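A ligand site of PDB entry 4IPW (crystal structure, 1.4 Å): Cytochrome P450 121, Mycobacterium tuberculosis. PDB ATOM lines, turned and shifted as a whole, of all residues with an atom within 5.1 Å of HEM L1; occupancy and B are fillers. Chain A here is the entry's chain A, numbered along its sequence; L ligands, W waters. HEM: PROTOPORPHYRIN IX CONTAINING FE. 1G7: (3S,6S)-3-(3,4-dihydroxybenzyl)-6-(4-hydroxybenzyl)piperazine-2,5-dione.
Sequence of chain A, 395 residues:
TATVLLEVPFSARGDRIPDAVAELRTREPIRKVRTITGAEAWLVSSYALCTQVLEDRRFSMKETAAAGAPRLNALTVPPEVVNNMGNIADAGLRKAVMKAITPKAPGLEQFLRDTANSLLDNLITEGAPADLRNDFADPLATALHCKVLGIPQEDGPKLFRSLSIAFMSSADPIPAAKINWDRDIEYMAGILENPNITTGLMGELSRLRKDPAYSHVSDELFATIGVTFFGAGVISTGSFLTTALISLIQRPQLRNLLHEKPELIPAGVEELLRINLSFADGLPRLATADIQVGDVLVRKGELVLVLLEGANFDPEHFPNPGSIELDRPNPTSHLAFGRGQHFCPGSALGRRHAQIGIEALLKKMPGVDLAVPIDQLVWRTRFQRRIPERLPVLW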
ATOM      1  N   LEU A  54     -21.162  -3.661 -21.729  1.00  0.00           N
ATOM      2  CA  LEU A  54     -19.903  -3.443 -22.472  1.00  0.00           C
ATOM      3  C   LEU A  54     -19.945  -2.188 -23.370  1.00  0.00           C
ATOM      4  O   LEU A  54     -18.878  -1.637 -23.664  1.00  0.00           O
ATOM      5  CB  LEU A  54     -19.545  -4.671 -23.331  1.00  0.00           C
ATOM      6  CG  LEU A  54     -19.230  -5.927 -22.525  1.00  0.00           C
ATOM      7  CD1 LEU A  54     -18.986  -7.114 -23.482  1.00  0.00           C
ATOM      8  CD2 LEU A  54     -17.992  -5.723 -21.629  1.00  0.00           C
ATOM      9  N   MET A  61     -13.426  -0.080 -16.981  1.00  0.00           N
ATOM     10  CA  MET A  61     -12.367  -1.033 -16.671  1.00  0.00           C
ATOM     11  C   MET A  61     -11.345  -0.340 -15.741  1.00  0.00           C
ATOM     12  O   MET A  61     -10.948  -0.892 -14.718  1.00  0.00           O
ATOM     13  CB  MET A  61     -11.653  -1.528 -17.955  1.00  0.00           C
ATOM     14  CG  MET A  61     -10.307  -2.303 -17.710  1.00  0.00           C
ATOM     15  SD  MET A  61     -10.397  -3.761 -16.529  1.00  0.00           S
ATOM     16  CE  MET A  61     -11.029  -5.020 -17.680  1.00  0.00           C
ATOM     17  N   ASN A  84      -4.297   0.181 -19.662  1.00  0.00           N
ATOM     18  CA  ASN A  84      -3.313   0.053 -20.735  1.00  0.00           C
ATOM     19  C   ASN A  84      -3.701   0.645 -22.069  1.00  0.00           C
ATOM     20  O   ASN A  84      -2.977   1.476 -22.616  1.00  0.00           O
ATOM     21  CB  ASN A  84      -2.926  -1.429 -20.924  1.00  0.00           C
ATOM     22  CG  ASN A  84      -1.634  -1.646 -21.696  1.00  0.00           C
ATOM     23  OD1 ASN A  84      -0.658  -0.904 -21.521  1.00  0.00           O
ATOM     24  ND2 ASN A  84      -1.568  -2.711 -22.475  1.00  0.00           N
ATOM     25  N   MET A  85      -4.850   0.237 -22.631  1.00  0.00           N
ATOM     26  CA  MET A  85      -5.198   0.764 -23.937  1.00  0.00           C
ATOM     27  C   MET A  85      -5.460   2.253 -23.916  1.00  0.00           C
ATOM     28  O   MET A  85      -5.102   2.953 -24.887  1.00  0.00           O
ATOM     29  CB  MET A  85      -6.300  -0.053 -24.593  1.00  0.00           C
ATOM     30  CG  MET A  85      -5.776  -1.309 -25.234  1.00  0.00           C
ATOM     31  SD  MET A  85      -4.914  -1.189 -26.827  1.00  0.00           S
ATOM     32  CE  MET A  85      -5.322   0.522 -27.376  1.00  0.00           C
ATOM     33  N   ILE A 101       0.124  -5.392 -35.340  1.00  0.00           N
ATOM     34  CA  ILE A 101      -0.467  -6.672 -34.934  1.00  0.00           C
ATOM     35  C   ILE A 101      -1.487  -7.277 -35.923  1.00  0.00           C
ATOM     36  O   ILE A 101      -2.140  -8.276 -35.602  1.00  0.00           O
ATOM     37  CB  ILE A 101      -0.934  -6.636 -33.457  1.00  0.00           C
ATOM     38  CG1 ILE A 101      -2.206  -5.808 -33.271  1.00  0.00           C
ATOM     39  CG2 ILE A 101       0.218  -6.172 -32.518  1.00  0.00           C
ATOM     40  CD1 ILE A 101      -2.810  -5.821 -31.855  1.00  0.00           C
ATOM     41  N   HIS A 145       3.932 -14.506 -31.532  1.00  0.00           N
ATOM     42  CA  HIS A 145       4.117 -13.236 -30.864  1.00  0.00           C
ATOM     43  C   HIS A 145       5.558 -12.732 -30.853  1.00  0.00           C
ATOM     44  O   HIS A 145       5.764 -11.515 -30.943  1.00  0.00           O
ATOM     45  CB  HIS A 145       3.457 -13.222 -29.485  1.00  0.00           C
ATOM     46  CG  HIS A 145       1.968 -13.195 -29.589  1.00  0.00           C
ATOM     47  ND1 HIS A 145       1.243 -14.336 -29.959  1.00  0.00           N
ATOM     48  CD2 HIS A 145       1.113 -12.126 -29.539  1.00  0.00           C
ATOM     49  CE1 HIS A 145      -0.031 -13.918 -30.076  1.00  0.00           C
ATOM     50  NE2 HIS A 145      -0.149 -12.605 -29.814  1.00  0.00           N
ATOM     51  N   PHE A 229       1.285  -6.870 -24.657  1.00  0.00           N
ATOM     52  CA  PHE A 229       0.783  -7.475 -25.902  1.00  0.00           C
ATOM     53  C   PHE A 229       1.330  -8.891 -26.067  1.00  0.00           C
ATOM     54  O   PHE A 229       0.600  -9.776 -26.536  1.00  0.00           O
ATOM     55  CB  PHE A 229       1.063  -6.554 -27.119  1.00  0.00           C
ATOM     56  CG  PHE A 229      -0.025  -5.510 -27.251  1.00  0.00           C
ATOM     57  CD1 PHE A 229      -0.184  -4.516 -26.278  1.00  0.00           C
ATOM     58  CD2 PHE A 229      -0.938  -5.560 -28.299  1.00  0.00           C
ATOM     59  CE1 PHE A 229      -1.239  -3.596 -26.348  1.00  0.00           C
ATOM     60  CE2 PHE A 229      -2.014  -4.640 -28.360  1.00  0.00           C
ATOM     61  CZ  PHE A 229      -2.122  -3.645 -27.415  1.00  0.00           C
ATOM     62  N   ALA A 232      -1.013 -10.887 -23.104  1.00  0.00           N
ATOM     63  CA  ALA A 232      -2.428 -11.081 -23.437  1.00  0.00           C
ATOM     64  C   ALA A 232      -2.568 -11.850 -24.758  1.00  0.00           C
ATOM     65  O   ALA A 232      -3.404 -12.744 -24.863  1.00  0.00           O
ATOM     66  CB  ALA A 232      -3.140  -9.716 -23.551  1.00  0.00           C
ATOM     67  N   GLY A 233      -1.730 -11.562 -25.752  1.00  0.00           N
ATOM     68  CA  GLY A 233      -1.882 -12.269 -27.027  1.00  0.00           C
ATOM     69  C   GLY A 233      -1.525 -13.728 -26.932  1.00  0.00           C
ATOM     70  O   GLY A 233      -2.251 -14.585 -27.467  1.00  0.00           O
ATOM     71  N   SER A 236      -4.101 -15.649 -24.767  1.00  0.00           N
ATOM     72  CA  SER A 236      -5.408 -15.734 -25.367  1.00  0.00           C
ATOM     73  C   SER A 236      -5.446 -16.640 -26.575  1.00  0.00           C
ATOM     74  O   SER A 236      -6.366 -17.477 -26.658  1.00  0.00           O
ATOM     75  CB  SER A 236      -5.943 -14.348 -25.726  1.00  0.00           C
ATOM     76  OG  SER A 236      -5.993 -13.508 -24.581  1.00  0.00           O
ATOM     77  N   THR A 237      -4.462 -16.530 -27.483  1.00  0.00           N
ATOM     78  CA  THR A 237      -4.394 -17.395 -28.664  1.00  0.00           C
ATOM     79  C   THR A 237      -4.059 -18.837 -28.308  1.00  0.00           C
ATOM     80  O   THR A 237      -4.653 -19.771 -28.856  1.00  0.00           O
ATOM     81  CB  THR A 237      -3.420 -16.849 -29.719  1.00  0.00           C
ATOM     82  OG1 THR A 237      -2.099 -16.735 -29.152  1.00  0.00           O
ATOM     83  CG2 THR A 237      -3.878 -15.514 -30.315  1.00  0.00           C
ATOM     84  N   PHE A 240      -7.256 -20.232 -26.439  1.00  0.00           N
ATOM     85  CA  PHE A 240      -8.373 -20.430 -27.339  1.00  0.00           C
ATOM     86  C   PHE A 240      -8.085 -21.589 -28.307  1.00  0.00           C
ATOM     87  O   PHE A 240      -8.949 -22.466 -28.460  1.00  0.00           O
ATOM     88  CB  PHE A 240      -8.674 -19.144 -28.147  1.00  0.00           C
ATOM     89  CG  PHE A 240      -9.671 -19.447 -29.223  1.00  0.00           C
ATOM     90  CD1 PHE A 240     -10.931 -19.929 -28.900  1.00  0.00           C
ATOM     91  CD2 PHE A 240      -9.313 -19.377 -30.574  1.00  0.00           C
ATOM     92  CE1 PHE A 240     -11.840 -20.316 -29.900  1.00  0.00           C
ATOM     93  CE2 PHE A 240     -10.205 -19.788 -31.569  1.00  0.00           C
ATOM     94  CZ  PHE A 240     -11.464 -20.263 -31.234  1.00  0.00           C
ATOM     95  N   LEU A 273     -15.107 -19.857 -31.732  1.00  0.00           N
ATOM     96  CA  LEU A 273     -14.977 -18.676 -30.863  1.00  0.00           C
ATOM     97  C   LEU A 273     -16.292 -18.485 -30.099  1.00  0.00           C
ATOM     98  O   LEU A 273     -16.300 -18.285 -28.880  1.00  0.00           O
ATOM     99  CB  LEU A 273     -14.687 -17.430 -31.737  1.00  0.00           C
ATOM    100  CG  LEU A 273     -13.224 -17.316 -32.188  1.00  0.00           C
ATOM    101  CD1 LEU A 273     -13.058 -16.341 -33.355  1.00  0.00           C
ATOM    102  CD2 LEU A 273     -12.342 -16.816 -31.014  1.00  0.00           C
ATOM    103  N   ASN A 276     -16.709 -20.872 -27.251  1.00  0.00           N
ATOM    104  CA  ASN A 276     -15.500 -21.045 -26.454  1.00  0.00           C
ATOM    105  C   ASN A 276     -15.702 -20.697 -24.988  1.00  0.00           C
ATOM    106  O   ASN A 276     -16.337 -19.694 -24.676  1.00  0.00           O
ATOM    107  CB  ASN A 276     -14.312 -20.300 -27.106  1.00  0.00           C
ATOM    108  CG  ASN A 276     -13.911 -18.994 -26.450  1.00  0.00           C
ATOM    109  OD1 ASN A 276     -13.257 -18.994 -25.396  1.00  0.00           O
ATOM    110  ND2 ASN A 276     -14.254 -17.854 -27.040  1.00  0.00           N
ATOM    111  N   PHE A 279     -12.462 -17.927 -21.392  1.00  0.00           N
ATOM    112  CA  PHE A 279     -12.438 -16.912 -20.312  1.00  0.00           C
ATOM    113  C   PHE A 279     -13.066 -17.495 -19.055  1.00  0.00           C
ATOM    114  O   PHE A 279     -14.257 -17.863 -19.040  1.00  0.00           O
ATOM    115  CB  PHE A 279     -13.123 -15.603 -20.740  1.00  0.00           C
ATOM    116  CG  PHE A 279     -12.183 -14.684 -21.492  1.00  0.00           C
ATOM    117  CD1 PHE A 279     -11.684 -15.055 -22.744  1.00  0.00           C
ATOM    118  CD2 PHE A 279     -11.811 -13.455 -20.961  1.00  0.00           C
ATOM    119  CE1 PHE A 279     -10.832 -14.190 -23.442  1.00  0.00           C
ATOM    120  CE2 PHE A 279     -10.902 -12.620 -21.654  1.00  0.00           C
ATOM    121  CZ  PHE A 279     -10.435 -13.002 -22.889  1.00  0.00           C
ATOM    122  N   LEU A 283     -16.070 -10.564 -17.579  1.00  0.00           N
ATOM    123  CA  LEU A 283     -15.241  -9.374 -17.761  1.00  0.00           C
ATOM    124  C   LEU A 283     -15.649  -8.354 -16.720  1.00  0.00           C
ATOM    125  O   LEU A 283     -16.843  -8.064 -16.587  1.00  0.00           O
ATOM    126  CB  LEU A 283     -15.445  -8.767 -19.164  1.00  0.00           C
ATOM    127  CG  LEU A 283     -15.173  -9.688 -20.351  1.00  0.00           C
ATOM    128  CD1 LEU A 283     -15.428  -8.927 -21.644  1.00  0.00           C
ATOM    129  CD2 LEU A 283     -13.707 -10.266 -20.318  1.00  0.00           C
ATOM    130  N   PRO A 284     -14.694  -7.795 -15.962  1.00  0.00           N
ATOM    131  CA  PRO A 284     -15.061  -6.904 -14.850  1.00  0.00           C
ATOM    132  C   PRO A 284     -15.170  -5.438 -15.251  1.00  0.00           C
ATOM    133  O   PRO A 284     -14.388  -4.949 -16.071  1.00  0.00           O
ATOM    134  CB  PRO A 284     -13.898  -7.105 -13.845  1.00  0.00           C
ATOM    135  CG  PRO A 284     -12.684  -7.379 -14.717  1.00  0.00           C
ATOM    136  CD  PRO A 284     -13.248  -8.142 -15.964  1.00  0.00           C
ATOM    137  N   ARG A 285     -16.123  -4.746 -14.631  1.00  0.00           N
ATOM    138  CA  ARG A 285     -16.299  -3.303 -14.794  1.00  0.00           C
ATOM    139  C   ARG A 285     -16.781  -2.724 -13.467  1.00  0.00           C
ATOM    140  O   ARG A 285     -17.524  -3.381 -12.741  1.00  0.00           O
ATOM    141  CB  ARG A 285     -17.371  -2.964 -15.852  1.00  0.00           C
ATOM    142  CG  ARG A 285     -17.098  -3.447 -17.277  1.00  0.00           C
ATOM    143  CD  ARG A 285     -15.902  -2.716 -17.880  1.00  0.00           C
ATOM    144  NE  ARG A 285     -15.772  -2.998 -19.322  1.00  0.00           N
ATOM    145  CZ  ARG A 285     -15.009  -3.965 -19.836  1.00  0.00           C
ATOM    146  NH1 ARG A 285     -14.301  -4.782 -19.032  1.00  0.00           N
ATOM    147  NH2 ARG A 285     -14.912  -4.107 -21.161  1.00  0.00           N
ATOM    148  N   LEU A 308     -19.213 -13.982 -20.625  1.00  0.00           N
ATOM    149  CA  LEU A 308     -19.197 -14.139 -22.091  1.00  0.00           C
ATOM    150  C   LEU A 308     -20.016 -15.310 -22.577  1.00  0.00           C
ATOM    151  O   LEU A 308     -20.713 -15.177 -23.598  1.00  0.00           O
ATOM    152  CB  LEU A 308     -17.765 -14.194 -22.639  1.00  0.00           C
ATOM    153  CG  LEU A 308     -16.928 -12.908 -22.360  1.00  0.00           C
ATOM    154  CD1 LEU A 308     -15.534 -13.028 -22.999  1.00  0.00           C
ATOM    155  CD2 LEU A 308     -17.649 -11.644 -22.874  1.00  0.00           C
ATOM    156  N   LEU A 335     -19.591 -12.378 -28.509  1.00  0.00           N
ATOM    157  CA  LEU A 335     -18.761 -11.541 -27.634  1.00  0.00           C
ATOM    158  C   LEU A 335     -17.417 -12.170 -27.269  1.00  0.00           C
ATOM    159  O   LEU A 335     -16.789 -11.765 -26.277  1.00  0.00           O
ATOM    160  CB  LEU A 335     -19.523 -11.171 -26.364  1.00  0.00           C
ATOM    161  CG  LEU A 335     -20.945 -10.585 -26.527  1.00  0.00           C
ATOM    162  CD1 LEU A 335     -21.414  -9.984 -25.215  1.00  0.00           C
ATOM    163  CD2 LEU A 335     -21.004  -9.473 -27.587  1.00  0.00           C
ATOM    164  N   ALA A 336     -16.898 -13.098 -28.084  1.00  0.00           N
ATOM    165  CA  ALA A 336     -15.626 -13.737 -27.725  1.00  0.00           C
ATOM    166  C   ALA A 336     -14.453 -12.745 -27.683  1.00  0.00           C
ATOM    167  O   ALA A 336     -13.490 -13.024 -26.955  1.00  0.00           O
ATOM    168  CB  ALA A 336     -15.300 -14.841 -28.760  1.00  0.00           C
ATOM    169  N   PHE A 337     -14.536 -11.632 -28.422  1.00  0.00           N
ATOM    170  CA  PHE A 337     -13.488 -10.603 -28.418  1.00  0.00           C
ATOM    171  C   PHE A 337     -13.997  -9.376 -27.639  1.00  0.00           C
ATOM    172  O   PHE A 337     -13.415  -8.296 -27.757  1.00  0.00           O
ATOM    173  CB  PHE A 337     -13.124 -10.200 -29.848  1.00  0.00           C
ATOM    174  CG  PHE A 337     -12.428 -11.311 -30.609  1.00  0.00           C
ATOM    175  CD1 PHE A 337     -11.175 -11.784 -30.198  1.00  0.00           C
ATOM    176  CD2 PHE A 337     -12.969 -11.826 -31.781  1.00  0.00           C
ATOM    177  CE1 PHE A 337     -10.518 -12.800 -30.905  1.00  0.00           C
ATOM    178  CE2 PHE A 337     -12.312 -12.845 -32.479  1.00  0.00           C
ATOM    179  CZ  PHE A 337     -11.090 -13.321 -32.038  1.00  0.00           C
ATOM    180  N   GLY A 338     -15.075  -9.521 -26.868  1.00  0.00           N
ATOM    181  CA  GLY A 338     -15.635  -8.381 -26.166  1.00  0.00           C
ATOM    182  C   GLY A 338     -16.512  -7.554 -27.078  1.00  0.00           C
ATOM    183  O   GLY A 338     -16.986  -8.014 -28.139  1.00  0.00           O
ATOM    184  N   GLN A 341     -15.723  -0.165 -26.156  1.00  0.00           N
ATOM    185  CA  GLN A 341     -14.440   0.520 -26.074  1.00  0.00           C
ATOM    186  C   GLN A 341     -13.261  -0.446 -25.969  1.00  0.00           C
ATOM    187  O   GLN A 341     -12.204  -0.149 -26.557  1.00  0.00           O
ATOM    188  CB  GLN A 341     -14.457   1.465 -24.869  1.00  0.00           C
ATOM    189  CG  GLN A 341     -13.171   2.265 -24.634  1.00  0.00           C
ATOM    190  CD  GLN A 341     -13.064   3.502 -25.498  1.00  0.00           C
ATOM    191  OE1 GLN A 341     -12.068   4.228 -25.471  1.00  0.00           O
ATOM    192  NE2 GLN A 341     -14.096   3.790 -26.268  1.00  0.00           N
ATOM    193  N   HIS A 342     -13.432  -1.579 -25.267  1.00  0.00           N
ATOM    194  CA  HIS A 342     -12.339  -2.504 -25.000  1.00  0.00           C
ATOM    195  C   HIS A 342     -12.310  -3.708 -25.941  1.00  0.00           C
ATOM    196  O   HIS A 342     -11.608  -4.685 -25.675  1.00  0.00           O
ATOM    197  CB  HIS A 342     -12.389  -2.969 -23.531  1.00  0.00           C
ATOM    198  CG  HIS A 342     -12.178  -1.846 -22.559  1.00  0.00           C
ATOM    199  ND1 HIS A 342     -10.908  -1.457 -22.182  1.00  0.00           N
ATOM    200  CD2 HIS A 342     -13.084  -1.040 -21.958  1.00  0.00           C
ATOM    201  CE1 HIS A 342     -11.080  -0.423 -21.354  1.00  0.00           C
ATOM    202  NE2 HIS A 342     -12.369  -0.158 -21.159  1.00  0.00           N
ATOM    203  N   PHE A 343     -13.020  -3.611 -27.096  1.00  0.00           N
ATOM    204  CA  PHE A 343     -13.006  -4.708 -28.082  1.00  0.00           C
ATOM    205  C   PHE A 343     -11.551  -5.092 -28.424  1.00  0.00           C
ATOM    206  O   PHE A 343     -10.694  -4.219 -28.603  1.00  0.00           O
ATOM    207  CB  PHE A 343     -13.769  -4.264 -29.337  1.00  0.00           C
ATOM    208  CG  PHE A 343     -13.855  -5.354 -30.377  1.00  0.00           C
ATOM    209  CD1 PHE A 343     -14.863  -6.310 -30.319  1.00  0.00           C
ATOM    210  CD2 PHE A 343     -12.891  -5.478 -31.377  1.00  0.00           C
ATOM    211  CE1 PHE A 343     -14.932  -7.347 -31.252  1.00  0.00           C
ATOM    212  CE2 PHE A 343     -12.934  -6.546 -32.286  1.00  0.00           C
ATOM    213  CZ  PHE A 343     -13.949  -7.474 -32.211  1.00  0.00           C
ATOM    214  N   CYS A 344     -11.255  -6.409 -28.399  1.00  0.00           N
ATOM    215  CA  CYS A 344      -9.919  -6.921 -28.593  1.00  0.00           C
ATOM    216  C   CYS A 344      -9.194  -6.286 -29.781  1.00  0.00           C
ATOM    217  O   CYS A 344      -9.632  -6.490 -30.919  1.00  0.00           O
ATOM    218  CB  CYS A 344      -9.960  -8.431 -28.778  1.00  0.00           C
ATOM    219  SG  CYS A 344      -8.299  -9.143 -28.927  1.00  0.00           S
ATOM    220  N   PRO A 345      -8.016  -5.696 -29.563  1.00  0.00           N
ATOM    221  CA  PRO A 345      -7.270  -5.125 -30.715  1.00  0.00           C
ATOM    222  C   PRO A 345      -6.569  -6.205 -31.519  1.00  0.00           C
ATOM    223  O   PRO A 345      -6.114  -5.918 -32.634  1.00  0.00           O
ATOM    224  CB  PRO A 345      -6.242  -4.188 -30.042  1.00  0.00           C
ATOM    225  CG  PRO A 345      -6.018  -4.804 -28.692  1.00  0.00           C
ATOM    226  CD  PRO A 345      -7.345  -5.396 -28.276  1.00  0.00           C
ATOM    227  N   GLY A 346      -6.457  -7.411 -30.957  1.00  0.00           N
ATOM    228  CA  GLY A 346      -5.800  -8.507 -31.675  1.00  0.00           C
ATOM    229  C   GLY A 346      -6.734  -9.502 -32.337  1.00  0.00           C
ATOM    230  O   GLY A 346      -6.283 -10.601 -32.704  1.00  0.00           O
ATOM    231  N   LEU A 349      -5.676 -11.141 -35.658  1.00  0.00           N
ATOM    232  CA  LEU A 349      -4.537 -12.029 -35.473  1.00  0.00           C
ATOM    233  C   LEU A 349      -4.924 -13.331 -34.773  1.00  0.00           C
ATOM    234  O   LEU A 349      -4.479 -14.400 -35.173  1.00  0.00           O
ATOM    235  CB  LEU A 349      -3.420 -11.315 -34.709  1.00  0.00           C
ATOM    236  CG  LEU A 349      -2.066 -12.036 -34.554  1.00  0.00           C
ATOM    237  CD1 LEU A 349      -1.360 -12.228 -35.914  1.00  0.00           C
ATOM    238  CD2 LEU A 349      -1.137 -11.279 -33.622  1.00  0.00           C
ATOM    239  N   GLY A 350      -5.809 -13.228 -33.774  1.00  0.00           N
ATOM    240  CA  GLY A 350      -6.308 -14.390 -33.033  1.00  0.00           C
ATOM    241  C   GLY A 350      -7.079 -15.318 -33.949  1.00  0.00           C
ATOM    242  O   GLY A 350      -6.902 -16.537 -33.884  1.00  0.00           O
HETATM  243  CHA HEM L   1      -8.957  -7.467 -24.843  1.00  0.00           C
HETATM  244  CHB HEM L   1     -10.293 -11.938 -26.195  1.00  0.00           C
HETATM  245  CHC HEM L   1      -6.214 -12.293 -28.827  1.00  0.00           C
HETATM  246  CHD HEM L   1      -4.568  -8.169 -26.868  1.00  0.00           C
HETATM  247  C1A HEM L   1      -9.734  -8.607 -25.071  1.00  0.00           C
HETATM  248  C2A HEM L   1     -11.076  -8.791 -24.612  1.00  0.00           C
HETATM  249  C3A HEM L   1     -11.419 -10.080 -24.930  1.00  0.00           C
HETATM  250  C4A HEM L   1     -10.330 -10.669 -25.652  1.00  0.00           C
HETATM  251  CMA HEM L   1     -12.738 -10.774 -24.602  1.00  0.00           C
HETATM  252  CAA HEM L   1     -11.921  -7.740 -23.863  1.00  0.00           C
HETATM  253  CBA HEM L   1     -11.597  -7.601 -22.385  1.00  0.00           C
HETATM  254  CGA HEM L   1     -12.538  -6.673 -21.714  1.00  0.00           C
HETATM  255  O1A HEM L   1     -13.360  -6.011 -22.346  1.00  0.00           O
HETATM  256  O2A HEM L   1     -12.384  -6.614 -20.399  1.00  0.00           O
HETATM  257  C1B HEM L   1      -9.225 -12.465 -26.985  1.00  0.00           C
HETATM  258  C2B HEM L   1      -9.321 -13.746 -27.651  1.00  0.00           C
HETATM  259  C3B HEM L   1      -8.173 -13.829 -28.425  1.00  0.00           C
HETATM  260  C4B HEM L   1      -7.423 -12.595 -28.144  1.00  0.00           C
HETATM  261  CMB HEM L   1     -10.453 -14.718 -27.510  1.00  0.00           C
HETATM  262  CAB HEM L   1      -7.708 -14.875 -29.356  1.00  0.00           C
HETATM  263  CBB HEM L   1      -8.380 -15.920 -29.761  1.00  0.00           C
HETATM  264  C1C HEM L   1      -5.450 -11.178 -28.575  1.00  0.00           C
HETATM  265  C2C HEM L   1      -4.175 -10.907 -29.211  1.00  0.00           C
HETATM  266  C3C HEM L   1      -3.701  -9.744 -28.641  1.00  0.00           C
HETATM  267  C4C HEM L   1      -4.700  -9.292 -27.681  1.00  0.00           C
HETATM  268  CMC HEM L   1      -3.519 -11.742 -30.286  1.00  0.00           C
HETATM  269  CAC HEM L   1      -2.434  -8.983 -28.922  1.00  0.00           C
HETATM  270  CBC HEM L   1      -1.424  -9.414 -29.649  1.00  0.00           C
HETATM  271  C1D HEM L   1      -5.593  -7.700 -26.081  1.00  0.00           C
HETATM  272  C2D HEM L   1      -5.522  -6.438 -25.327  1.00  0.00           C
HETATM  273  C3D HEM L   1      -6.782  -6.170 -24.883  1.00  0.00           C
HETATM  274  C4D HEM L   1      -7.621  -7.332 -25.274  1.00  0.00           C
HETATM  275  CMD HEM L   1      -4.279  -5.592 -25.165  1.00  0.00           C
HETATM  276  CAD HEM L   1      -7.295  -4.967 -24.048  1.00  0.00           C
HETATM  277  CBD HEM L   1      -8.025  -3.954 -24.947  1.00  0.00           C
HETATM  278  CGD HEM L   1      -8.675  -2.733 -24.310  1.00  0.00           C
HETATM  279  O1D HEM L   1      -9.143  -1.854 -24.994  1.00  0.00           O
HETATM  280  O2D HEM L   1      -8.692  -2.754 -23.003  1.00  0.00           O
HETATM  281  NA  HEM L   1      -9.274  -9.736 -25.765  1.00  0.00           N
HETATM  282  NB  HEM L   1      -8.084 -11.808 -27.279  1.00  0.00           N
HETATM  283  NC  HEM L   1      -5.767 -10.166 -27.708  1.00  0.00           N
HETATM  284  ND  HEM L   1      -6.885  -8.214 -25.974  1.00  0.00           N
HETATM  285 FE   HEM L   1      -7.558  -9.902 -26.824  1.00  0.00          FE
HETATM  286  OB  1G7 L   2      -3.704  -4.640 -21.801  1.00  0.00           O
HETATM  287  CB  1G7 L   2      -4.140  -4.782 -20.648  1.00  0.00           C
HETATM  288  CAB 1G7 L   2      -3.375  -5.685 -19.709  1.00  0.00           C
HETATM  289  CBB 1G7 L   2      -3.502  -7.187 -20.196  1.00  0.00           C
HETATM  290  CGB 1G7 L   2      -2.453  -8.014 -19.409  1.00  0.00           C
HETATM  291  CD4 1G7 L   2      -2.815  -8.647 -18.173  1.00  0.00           C
HETATM  292  CE4 1G7 L   2      -1.854  -9.314 -17.474  1.00  0.00           C
HETATM  293  OH4 1G7 L   2      -2.188  -9.968 -16.294  1.00  0.00           O
HETATM  294  CZB 1G7 L   2      -0.541  -9.420 -17.926  1.00  0.00           C
HETATM  295  OHB 1G7 L   2       0.421 -10.076 -17.151  1.00  0.00           O
HETATM  296  CE3 1G7 L   2      -0.177  -8.850 -19.199  1.00  0.00           C
HETATM  297  CD3 1G7 L   2      -1.184  -8.157 -19.935  1.00  0.00           C
HETATM  298  NB  1G7 L   2      -3.817  -5.622 -18.307  1.00  0.00           N
HETATM  299  CA  1G7 L   2      -4.899  -5.008 -17.837  1.00  0.00           C
HETATM  300  OA  1G7 L   2      -5.224  -4.993 -16.628  1.00  0.00           O
HETATM  301  NA  1G7 L   2      -5.210  -4.149 -20.183  1.00  0.00           N
HETATM  302  CAA 1G7 L   2      -5.784  -4.243 -18.828  1.00  0.00           C
HETATM  303  CBA 1G7 L   2      -7.163  -4.893 -18.874  1.00  0.00           C
HETATM  304  CGA 1G7 L   2      -7.120  -6.330 -19.377  1.00  0.00           C
HETATM  305  CD1 1G7 L   2      -7.142  -6.683 -20.710  1.00  0.00           C
HETATM  306  CE1 1G7 L   2      -7.090  -7.982 -21.230  1.00  0.00           C
HETATM  307  CZA 1G7 L   2      -6.982  -9.040 -20.278  1.00  0.00           C
HETATM  308  OHA 1G7 L   2      -6.938 -10.316 -20.719  1.00  0.00           O
HETATM  309  CE2 1G7 L   2      -6.941  -8.697 -18.916  1.00  0.00           C
HETATM  310  CD2 1G7 L   2      -6.990  -7.384 -18.455  1.00  0.00           C
HETATM  311  O   HOH W   1      -6.574  -1.963 -21.532  1.00  0.00           O
HETATM  312  O   HOH W   2      -6.669 -10.839 -24.791  1.00  0.00           O
HETATM  313  O   HOH W   3     -14.811  -5.591 -24.590  1.00  0.00           O
HETATM  314  O   HOH W   4      -9.129  -2.124 -27.648  1.00  0.00           O
HETATM  315  O   HOH W   5     -10.424  -7.985 -19.152  1.00  0.00           O
HETATM  316  O   HOH W   6      -8.378 -10.550 -22.822  1.00  0.00           O
HETATM  317  O   HOH W   7      -9.874   0.707 -24.335  1.00  0.00           O
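N of Cys 344 sits at hydrogen-bond distance from O of Phe 337. O of Gly 233 is in hydrogen-bond range of OG1 of Thr 237 (2.7 Å). The side-chain hydroxyl (OG) of Ser 236 lies within hydrogen-bond range of the backbone carbonyl oxygen (O) of Ala 232, 2.7 Å away. N of Gly 346 lies close to SG of Cys 344.
Met 61 touches HEM L1 (CE to O2A, 3.4 Å). Met 85 touches HEM L1 (CG to CGD, 3.4 Å). NE2 of His 145 touches CBC of HEM L1, at 3.4 Å. Phe 229 touches HEM L1. Ala 232 touches HEM L1 (CB to CHD, 3.9 Å). Gly 233 touches HEM L1. CB of Ser 236 touches C4B of HEM L1 (3.3 Å). Thr 237 touches HEM L1. Phe 240 touches HEM L1 (CB to CBB, 3.6 Å). Phe 279 touches HEM L1. CD1 of Leu 283 touches O1A of HEM L1, at 3.6 Å. CD1 of Leu 308 touches CMA of HEM L1 (3.9 Å). O of Ala 336 touches CMA of HEM L1 (3.3 Å). Phe 337 touches HEM L1. N of Gly 338 touches CMA of HEM L1, at 3.5 Å. Gln 341 touches HEM L1 (O to O1D, 3.8 Å). Pro 345 touches HEM L1 (CD to C3D, 3.5 Å). Gly 346 touches HEM L1 (CA to C2C, 3.8 Å). Gly 350 touches HEM L1 (CA to CAB, 3.96 Å). Hydrophobic or aromatic side chains that line HEM L1: Met 61, Met 85, His 145, Phe 229, Ala 232, Phe 240, Phe 279, Leu 283, Leu 308, Phe 337, His 342 and Pro 345. 22 residues have an atom within 4 Å of HEM L1: Met 61, Met 85, His 145, Phe 229, Ala 232, Gly 233, Ser 236, Thr 237, Phe 240, Phe 279, Leu 283, Arg 285, Leu 308, Ala 336, Phe 337, Gly 338, Gln 341, His 342, Cys 344, Pro 345, Gly 346 and Gly 350. The nearest printed residue that does not touch HEM L1 is Leu 349 (4.1 Å).
The side-chain sulfur (SG) of Cys 344 binds an iron atom (FE) of HEM L1. An oxygen (O2D) of HEM L1 is in hydrogen-bond range of a ring nitrogen (ND1) of His 342 (2.7 Å). ND2 of Asn 84 lies within hydrogen-bond range of OB of 1G7 L2, 3.0 Å away. An oxygen (O1A) of HEM L1 is in salt-bridge range of the guanidinium group (NH2) of Arg 285 (2.7 Å).
Water W4 bridges O1D of HEM L1 and O of Phe 343. Water W1 lies within hydrogen-bond range of O2D of HEM L1 (2.7 Å), NA of 1G7 L2 (2.9 Å) and N of Met 85 (3.0 Å). Water W7 lies within hydrogen-bond range of O1D of HEM L1 (2.7 Å), ND1 of His 342 (3.2 Å) and O of Gln 341 (3.3 Å).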
